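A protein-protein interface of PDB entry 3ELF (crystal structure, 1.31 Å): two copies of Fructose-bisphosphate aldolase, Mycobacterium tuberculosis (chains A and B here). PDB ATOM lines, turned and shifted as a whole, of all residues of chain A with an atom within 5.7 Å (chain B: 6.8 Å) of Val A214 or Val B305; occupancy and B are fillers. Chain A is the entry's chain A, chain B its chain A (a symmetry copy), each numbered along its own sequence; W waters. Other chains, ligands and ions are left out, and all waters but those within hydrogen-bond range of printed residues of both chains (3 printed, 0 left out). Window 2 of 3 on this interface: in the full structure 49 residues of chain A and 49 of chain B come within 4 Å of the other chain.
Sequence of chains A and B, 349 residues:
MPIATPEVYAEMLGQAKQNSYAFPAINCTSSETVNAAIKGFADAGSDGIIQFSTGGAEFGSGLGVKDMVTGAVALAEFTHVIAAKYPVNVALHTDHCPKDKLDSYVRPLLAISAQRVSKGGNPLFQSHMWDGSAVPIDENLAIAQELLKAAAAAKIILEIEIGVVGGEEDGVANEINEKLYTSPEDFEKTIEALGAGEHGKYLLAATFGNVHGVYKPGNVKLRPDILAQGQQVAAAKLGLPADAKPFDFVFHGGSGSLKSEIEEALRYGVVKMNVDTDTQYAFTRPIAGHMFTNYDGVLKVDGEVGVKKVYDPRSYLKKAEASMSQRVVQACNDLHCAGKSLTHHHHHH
OG of Ser A255 sits at hydrogen-bond distance from N of Thr A277, 3.3 Å away.
The side-chain amino group (NZ) of Lys B308 lies within hydrogen-bond range of the side-chain hydroxyl (OG1) of Thr A277, at 2.8 Å.
The backbone NH of Lys B300 lies within hydrogen-bond range of the side-chain hydroxyl of Tyr A281 (3.1 Å).
NZ of Lys A216 lies within salt-bridge range of OE1 of Glu B304.
Val A214 touches Val B305 (O to CG2, 3.7 Å).
CG2 of Thr A277 touches OH of Tyr B311 (3.1 Å).
CA of Leu B299 touches OH of Tyr A281, at 3.9 Å.
Tyr B311 touches Tyr A281.
Of the printed residues of chain B, Lys A216 touches Glu B304.
Of the printed residues of chain B, Thr A277 touches Lys B308 (2.8 Å) and Tyr B311 (3.1 Å).
Printed residues of chain B within 4 Å of Tyr A281: Leu B299, Lys B300 and Tyr B311.
Of the printed residues of chain A, Glu B304 touches Lys A216.
Of chain A, only Val A214 (3.7 Å) comes within 4 Å of Val B305.
The nearest residue of chain B that does not touch Val A214 is Tyr B311 (4.1 Å).
The nearest residue of chain A that does not touch Val B305 is Lys A216 (4.02 Å).
Hydrophobic or aromatic side chains of chain B within 4 Å of the printed part of chain A: Val B305 and Tyr B311.
Printed residues of chain A that touch a printed residue of chain B: Val A214, Lys A216, Thr A277 and Tyr A281.
Along chain A the printed residues that touch a printed residue of chain B span positions 214 to 281.
No position is printed for both chains.
Of the 7 pairs that touch across the chains among the printed residues, none has its exchanged pair printed and touching as well.
Water W1 lies within hydrogen-bond range of O of Val B305 (2.7 Å), OH of Tyr B311 (2.7 Å) and O of Val A214 (3.2 Å).
Water W3 bridges OD1 of Asp A278 and NZ of Lys B300.
Water W2 lies within hydrogen-bond range of NZ of Lys B300, OD1 of Asp A278 and OH of Tyr B311.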
ATOM      1  N   HIS A 212      22.545  -0.609   2.274  1.00  0.00           N
ATOM      2  CA  HIS A 212      21.872  -0.747   3.567  1.00  0.00           C
ATOM      3  C   HIS A 212      20.562   0.033   3.528  1.00  0.00           C
ATOM      4  O   HIS A 212      20.541   1.176   3.062  1.00  0.00           O
ATOM      5  CB  HIS A 212      22.728  -0.158   4.686  1.00  0.00           C
ATOM      6  CG  HIS A 212      23.978  -0.926   4.986  1.00  0.00           C
ATOM      7  ND1 HIS A 212      25.225  -0.346   4.944  1.00  0.00           N
ATOM      8  CD2 HIS A 212      24.171  -2.208   5.367  1.00  0.00           C
ATOM      9  CE1 HIS A 212      26.137  -1.244   5.277  1.00  0.00           C
ATOM     10  NE2 HIS A 212      25.521  -2.378   5.553  1.00  0.00           N
ATOM     11  N   GLY A 213      19.497  -0.564   4.052  1.00  0.00           N
ATOM     12  CA  GLY A 213      18.189   0.082   4.086  1.00  0.00           C
ATOM     13  C   GLY A 213      17.204  -0.549   3.123  1.00  0.00           C
ATOM     14  O   GLY A 213      17.555  -1.460   2.365  1.00  0.00           O
ATOM     15  N   VAL A 214      15.970  -0.059   3.154  1.00  0.00           N
ATOM     16  CA  VAL A 214      14.905  -0.575   2.302  1.00  0.00           C
ATOM     17  C   VAL A 214      14.276   0.556   1.511  1.00  0.00           C
ATOM     18  O   VAL A 214      13.745   1.509   2.083  1.00  0.00           O
ATOM     19  CB  VAL A 214      13.822  -1.322   3.125  1.00  0.00           C
ATOM     20  CG1 VAL A 214      12.577  -1.619   2.278  1.00  0.00           C
ATOM     21  CG2 VAL A 214      14.401  -2.599   3.681  1.00  0.00           C
ATOM     22  N   TYR A 215      14.342   0.421   0.192  1.00  0.00           N
ATOM     23  CA  TYR A 215      13.845   1.428  -0.737  1.00  0.00           C
ATOM     24  C   TYR A 215      12.786   0.786  -1.622  1.00  0.00           C
ATOM     25  O   TYR A 215      12.564  -0.426  -1.546  1.00  0.00           O
ATOM     26  CB  TYR A 215      15.023   1.993  -1.547  1.00  0.00           C
ATOM     27  CG  TYR A 215      16.175   2.358  -0.640  1.00  0.00           C
ATOM     28  CD1 TYR A 215      17.107   1.396  -0.249  1.00  0.00           C
ATOM     29  CD2 TYR A 215      16.296   3.647  -0.118  1.00  0.00           C
ATOM     30  CE1 TYR A 215      18.142   1.709   0.613  1.00  0.00           C
ATOM     31  CE2 TYR A 215      17.340   3.972   0.744  1.00  0.00           C
ATOM     32  CZ  TYR A 215      18.252   2.995   1.104  1.00  0.00           C
ATOM     33  OH  TYR A 215      19.285   3.296   1.956  1.00  0.00           O
ATOM     34  N   LYS A 216      12.120   1.598  -2.438  1.00  0.00           N
ATOM     35  CA  LYS A 216      11.091   1.108  -3.357  1.00  0.00           C
ATOM     36  C   LYS A 216      11.683   0.126  -4.369  1.00  0.00           C
ATOM     37  O   LYS A 216      12.857   0.248  -4.726  1.00  0.00           O
ATOM     38  CB  LYS A 216      10.418   2.275  -4.078  1.00  0.00           C
ATOM     39  CG  LYS A 216       9.425   3.032  -3.214  1.00  0.00           C
ATOM     40  CD  LYS A 216       8.737   4.133  -3.996  1.00  0.00           C
ATOM     41  CE  LYS A 216       7.736   4.867  -3.128  1.00  0.00           C
ATOM     42  NZ  LYS A 216       7.183   6.055  -3.830  1.00  0.00           N
ATOM     43  N   PRO A 217      10.877  -0.857  -4.824  1.00  0.00           N
ATOM     44  CA  PRO A 217      11.381  -1.838  -5.794  1.00  0.00           C
ATOM     45  C   PRO A 217      11.926  -1.180  -7.060  1.00  0.00           C
ATOM     46  O   PRO A 217      11.286  -0.289  -7.626  1.00  0.00           O
ATOM     47  CB  PRO A 217      10.144  -2.683  -6.116  1.00  0.00           C
ATOM     48  CG  PRO A 217       9.274  -2.541  -4.917  1.00  0.00           C
ATOM     49  CD  PRO A 217       9.473  -1.127  -4.459  1.00  0.00           C
ATOM     50  N   SER A 255      18.164  -6.621   3.249  1.00  0.00           N
ATOM     51  CA  SER A 255      16.742  -6.274   3.314  1.00  0.00           C
ATOM     52  C   SER A 255      16.275  -5.629   2.022  1.00  0.00           C
ATOM     53  O   SER A 255      17.005  -4.840   1.419  1.00  0.00           O
ATOM     54  CB  SER A 255      16.458  -5.321   4.467  1.00  0.00           C
ATOM     55  OG  SER A 255      16.755  -5.913   5.720  1.00  0.00           O
ATOM     56  N   GLY A 256      15.061  -5.968   1.597  1.00  0.00           N
ATOM     57  CA  GLY A 256      14.459  -5.327   0.432  1.00  0.00           C
ATOM     58  C   GLY A 256      14.879  -5.896  -0.906  1.00  0.00           C
ATOM     59  O   GLY A 256      14.392  -5.447  -1.941  1.00  0.00           O
ATOM     60  N   THR A 277      17.099  -4.128   8.481  1.00  0.00           N
ATOM     61  CA  THR A 277      15.947  -3.261   8.270  1.00  0.00           C
ATOM     62  C   THR A 277      14.620  -4.033   8.182  1.00  0.00           C
ATOM     63  O   THR A 277      13.622  -3.640   8.797  1.00  0.00           O
ATOM     64  CB  THR A 277      16.174  -2.366   7.040  1.00  0.00           C
ATOM     65  OG1 THR A 277      17.383  -1.621   7.218  1.00  0.00           O
ATOM     66  CG2 THR A 277      15.040  -1.378   6.884  1.00  0.00           C
ATOM     67  N   ASP A 278      14.601  -5.140   7.448  1.00  0.00           N
ATOM     68  CA  ASP A 278      13.368  -5.899   7.296  1.00  0.00           C
ATOM     69  C   ASP A 278      12.913  -6.565   8.596  1.00  0.00           C
ATOM     70  O   ASP A 278      11.714  -6.678   8.850  1.00  0.00           O
ATOM     71  CB  ASP A 278      13.487  -6.934   6.175  1.00  0.00           C
ATOM     72  CG  ASP A 278      13.192  -6.354   4.792  1.00  0.00           C
ATOM     73  OD1 ASP A 278      12.723  -5.197   4.688  1.00  0.00           O
ATOM     74  OD2 ASP A 278      13.440  -7.080   3.803  1.00  0.00           O
ATOM     75  N   TYR A 281      11.369  -3.795  10.738  1.00  0.00           N
ATOM     76  CA  TYR A 281       9.986  -3.530  10.370  1.00  0.00           C
ATOM     77  C   TYR A 281       9.069  -4.615  10.921  1.00  0.00           C
ATOM     78  O   TYR A 281       7.999  -4.314  11.451  1.00  0.00           O
ATOM     79  CB  TYR A 281       9.803  -3.402   8.849  1.00  0.00           C
ATOM     80  CG  TYR A 281       8.383  -3.005   8.490  1.00  0.00           C
ATOM     81  CD1 TYR A 281       7.929  -1.709   8.724  1.00  0.00           C
ATOM     82  CD2 TYR A 281       7.485  -3.929   7.968  1.00  0.00           C
ATOM     83  CE1 TYR A 281       6.633  -1.330   8.425  1.00  0.00           C
ATOM     84  CE2 TYR A 281       6.170  -3.558   7.655  1.00  0.00           C
ATOM     85  CZ  TYR A 281       5.754  -2.255   7.896  1.00  0.00           C
ATOM     86  OH  TYR A 281       4.471  -1.853   7.607  1.00  0.00           O
ATOM     87  N   ASP B 296       3.039   7.164   9.894  1.00  0.00           N
ATOM     88  CA  ASP B 296       3.328   6.946   8.474  1.00  0.00           C
ATOM     89  C   ASP B 296       4.786   6.570   8.227  1.00  0.00           C
ATOM     90  O   ASP B 296       5.206   6.401   7.080  1.00  0.00           O
ATOM     91  CB  ASP B 296       2.877   8.139   7.608  1.00  0.00           C
ATOM     92  CG  ASP B 296       3.435   9.470   8.075  1.00  0.00           C
ATOM     93  OD1 ASP B 296       4.136   9.514   9.109  1.00  0.00           O
ATOM     94  OD2 ASP B 296       3.151  10.487   7.394  1.00  0.00           O
ATOM     95  N   GLY B 297       5.539   6.427   9.312  1.00  0.00           N
ATOM     96  CA  GLY B 297       6.906   5.916   9.253  1.00  0.00           C
ATOM     97  C   GLY B 297       6.996   4.491   9.769  1.00  0.00           C
ATOM     98  O   GLY B 297       7.767   3.681   9.240  1.00  0.00           O
ATOM     99  N   LEU B 299       4.395   2.455   9.737  1.00  0.00           N
ATOM    100  CA  LEU B 299       3.563   1.688   8.821  1.00  0.00           C
ATOM    101  C   LEU B 299       3.938   2.031   7.394  1.00  0.00           C
ATOM    102  O   LEU B 299       4.233   3.188   7.087  1.00  0.00           O
ATOM    103  CB  LEU B 299       2.086   2.022   9.024  1.00  0.00           C
ATOM    104  CG  LEU B 299       1.477   1.814  10.415  1.00  0.00           C
ATOM    105  CD1 LEU B 299       0.043   2.340  10.445  1.00  0.00           C
ATOM    106  CD2 LEU B 299       1.532   0.345  10.852  1.00  0.00           C
ATOM    107  N   LYS B 300       3.905   1.020   6.532  1.00  0.00           N
ATOM    108  CA  LYS B 300       4.070   1.219   5.093  1.00  0.00           C
ATOM    109  C   LYS B 300       2.696   1.564   4.538  1.00  0.00           C
ATOM    110  O   LYS B 300       1.835   0.697   4.398  1.00  0.00           O
ATOM    111  CB  LYS B 300       4.651  -0.041   4.457  1.00  0.00           C
ATOM    112  CG  LYS B 300       6.081  -0.283   4.910  1.00  0.00           C
ATOM    113  CD  LYS B 300       6.673  -1.568   4.366  1.00  0.00           C
ATOM    114  CE  LYS B 300       8.102  -1.728   4.887  1.00  0.00           C
ATOM    115  NZ  LYS B 300       8.790  -2.935   4.347  1.00  0.00           N
ATOM    116  N   VAL B 301       2.488   2.850   4.271  1.00  0.00           N
ATOM    117  CA  VAL B 301       1.162   3.352   3.922  1.00  0.00           C
ATOM    118  C   VAL B 301       1.131   3.919   2.498  1.00  0.00           C
ATOM    119  O   VAL B 301       2.103   4.531   2.036  1.00  0.00           O
ATOM    120  CB  VAL B 301       0.653   4.373   4.997  1.00  0.00           C
ATOM    121  CG1 VAL B 301       1.667   5.471   5.249  1.00  0.00           C
ATOM    122  CG2 VAL B 301      -0.716   4.955   4.653  1.00  0.00           C
ATOM    123  N   GLY B 303       1.427   2.761  -0.428  1.00  0.00           N
ATOM    124  CA  GLY B 303       2.462   2.314  -1.356  1.00  0.00           C
ATOM    125  C   GLY B 303       3.873   2.734  -0.992  1.00  0.00           C
ATOM    126  O   GLY B 303       4.814   2.392  -1.707  1.00  0.00           O
ATOM    127  N   GLU B 304       4.025   3.472   0.106  1.00  0.00           N
ATOM    128  CA  GLU B 304       5.338   3.905   0.583  1.00  0.00           C
ATOM    129  C   GLU B 304       5.990   2.805   1.421  1.00  0.00           C
ATOM    130  O   GLU B 304       5.336   1.822   1.785  1.00  0.00           O
ATOM    131  CB  GLU B 304       5.228   5.216   1.373  1.00  0.00           C
ATOM    132  CG  GLU B 304       4.568   6.377   0.606  1.00  0.00           C
ATOM    133  CD  GLU B 304       5.322   6.803  -0.646  1.00  0.00           C
ATOM    134  OE1 GLU B 304       6.570   6.812  -0.637  1.00  0.00           O
ATOM    135  OE2 GLU B 304       4.656   7.148  -1.645  1.00  0.00           O
ATOM    136  N   VAL B 305       7.276   2.966   1.720  1.00  0.00           N
ATOM    137  CA  VAL B 305       8.035   1.913   2.401  1.00  0.00           C
ATOM    138  C   VAL B 305       8.350   2.221   3.868  1.00  0.00           C
ATOM    139  O   VAL B 305       9.215   1.583   4.467  1.00  0.00           O
ATOM    140  CB  VAL B 305       9.338   1.535   1.622  1.00  0.00           C
ATOM    141  CG1 VAL B 305       8.996   1.013   0.240  1.00  0.00           C
ATOM    142  CG2 VAL B 305      10.315   2.718   1.534  1.00  0.00           C
ATOM    143  N   GLY B 306       7.632   3.175   4.459  1.00  0.00           N
ATOM    144  CA  GLY B 306       7.899   3.549   5.844  1.00  0.00           C
ATOM    145  C   GLY B 306       9.217   4.283   5.976  1.00  0.00           C
ATOM    146  O   GLY B 306       9.834   4.667   4.980  1.00  0.00           O
ATOM    147  N   VAL B 307       9.648   4.461   7.218  1.00  0.00           N
ATOM    148  CA  VAL B 307      10.840   5.245   7.520  1.00  0.00           C
ATOM    149  C   VAL B 307      11.653   4.470   8.550  1.00  0.00           C
ATOM    150  O   VAL B 307      11.284   4.389   9.727  1.00  0.00           O
ATOM    151  CB  VAL B 307      10.476   6.656   8.050  1.00  0.00           C
ATOM    152  CG1 VAL B 307      11.733   7.439   8.445  1.00  0.00           C
ATOM    153  CG2 VAL B 307       9.676   7.433   6.997  1.00  0.00           C
ATOM    154  N   LYS B 308      12.761   3.888   8.095  1.00  0.00           N
ATOM    155  CA  LYS B 308      13.596   3.039   8.944  1.00  0.00           C
ATOM    156  C   LYS B 308      13.987   3.697  10.256  1.00  0.00           C
ATOM    157  O   LYS B 308      13.981   3.045  11.297  1.00  0.00           O
ATOM    158  CB  LYS B 308      14.858   2.620   8.180  1.00  0.00           C
ATOM    159  CG  LYS B 308      15.919   1.927   9.031  1.00  0.00           C
ATOM    160  CD  LYS B 308      17.196   1.718   8.222  1.00  0.00           C
ATOM    161  CE  LYS B 308      18.332   1.202   9.093  1.00  0.00           C
ATOM    162  NZ  LYS B 308      18.080  -0.195   9.538  1.00  0.00           N
ATOM    163  N   TYR B 311      11.112   3.063  12.582  1.00  0.00           N
ATOM    164  CA  TYR B 311      10.737   1.684  12.879  1.00  0.00           C
ATOM    165  C   TYR B 311      11.885   0.837  13.424  1.00  0.00           C
ATOM    166  O   TYR B 311      11.671  -0.280  13.872  1.00  0.00           O
ATOM    167  CB  TYR B 311       9.939   1.017  11.753  1.00  0.00           C
ATOM    168  CG  TYR B 311      10.587   0.711  10.424  1.00  0.00           C
ATOM    169  CD1 TYR B 311      11.557  -0.284  10.297  1.00  0.00           C
ATOM    170  CD2 TYR B 311      10.147   1.351   9.257  1.00  0.00           C
ATOM    171  CE1 TYR B 311      12.091  -0.610   9.051  1.00  0.00           C
ATOM    172  CE2 TYR B 311      10.667   1.024   8.009  1.00  0.00           C
ATOM    173  CZ  TYR B 311      11.641   0.049   7.916  1.00  0.00           C
ATOM    174  OH  TYR B 311      12.161  -0.296   6.692  1.00  0.00           O
HETATM  175  O   HOH W   1      11.859   1.367   4.617  1.00  0.00           O
HETATM  176  O   HOH W   2      11.247  -3.004   5.708  1.00  0.00           O
HETATM  177  O   HOH W   3      10.836  -5.076   2.774  1.00  0.00           O
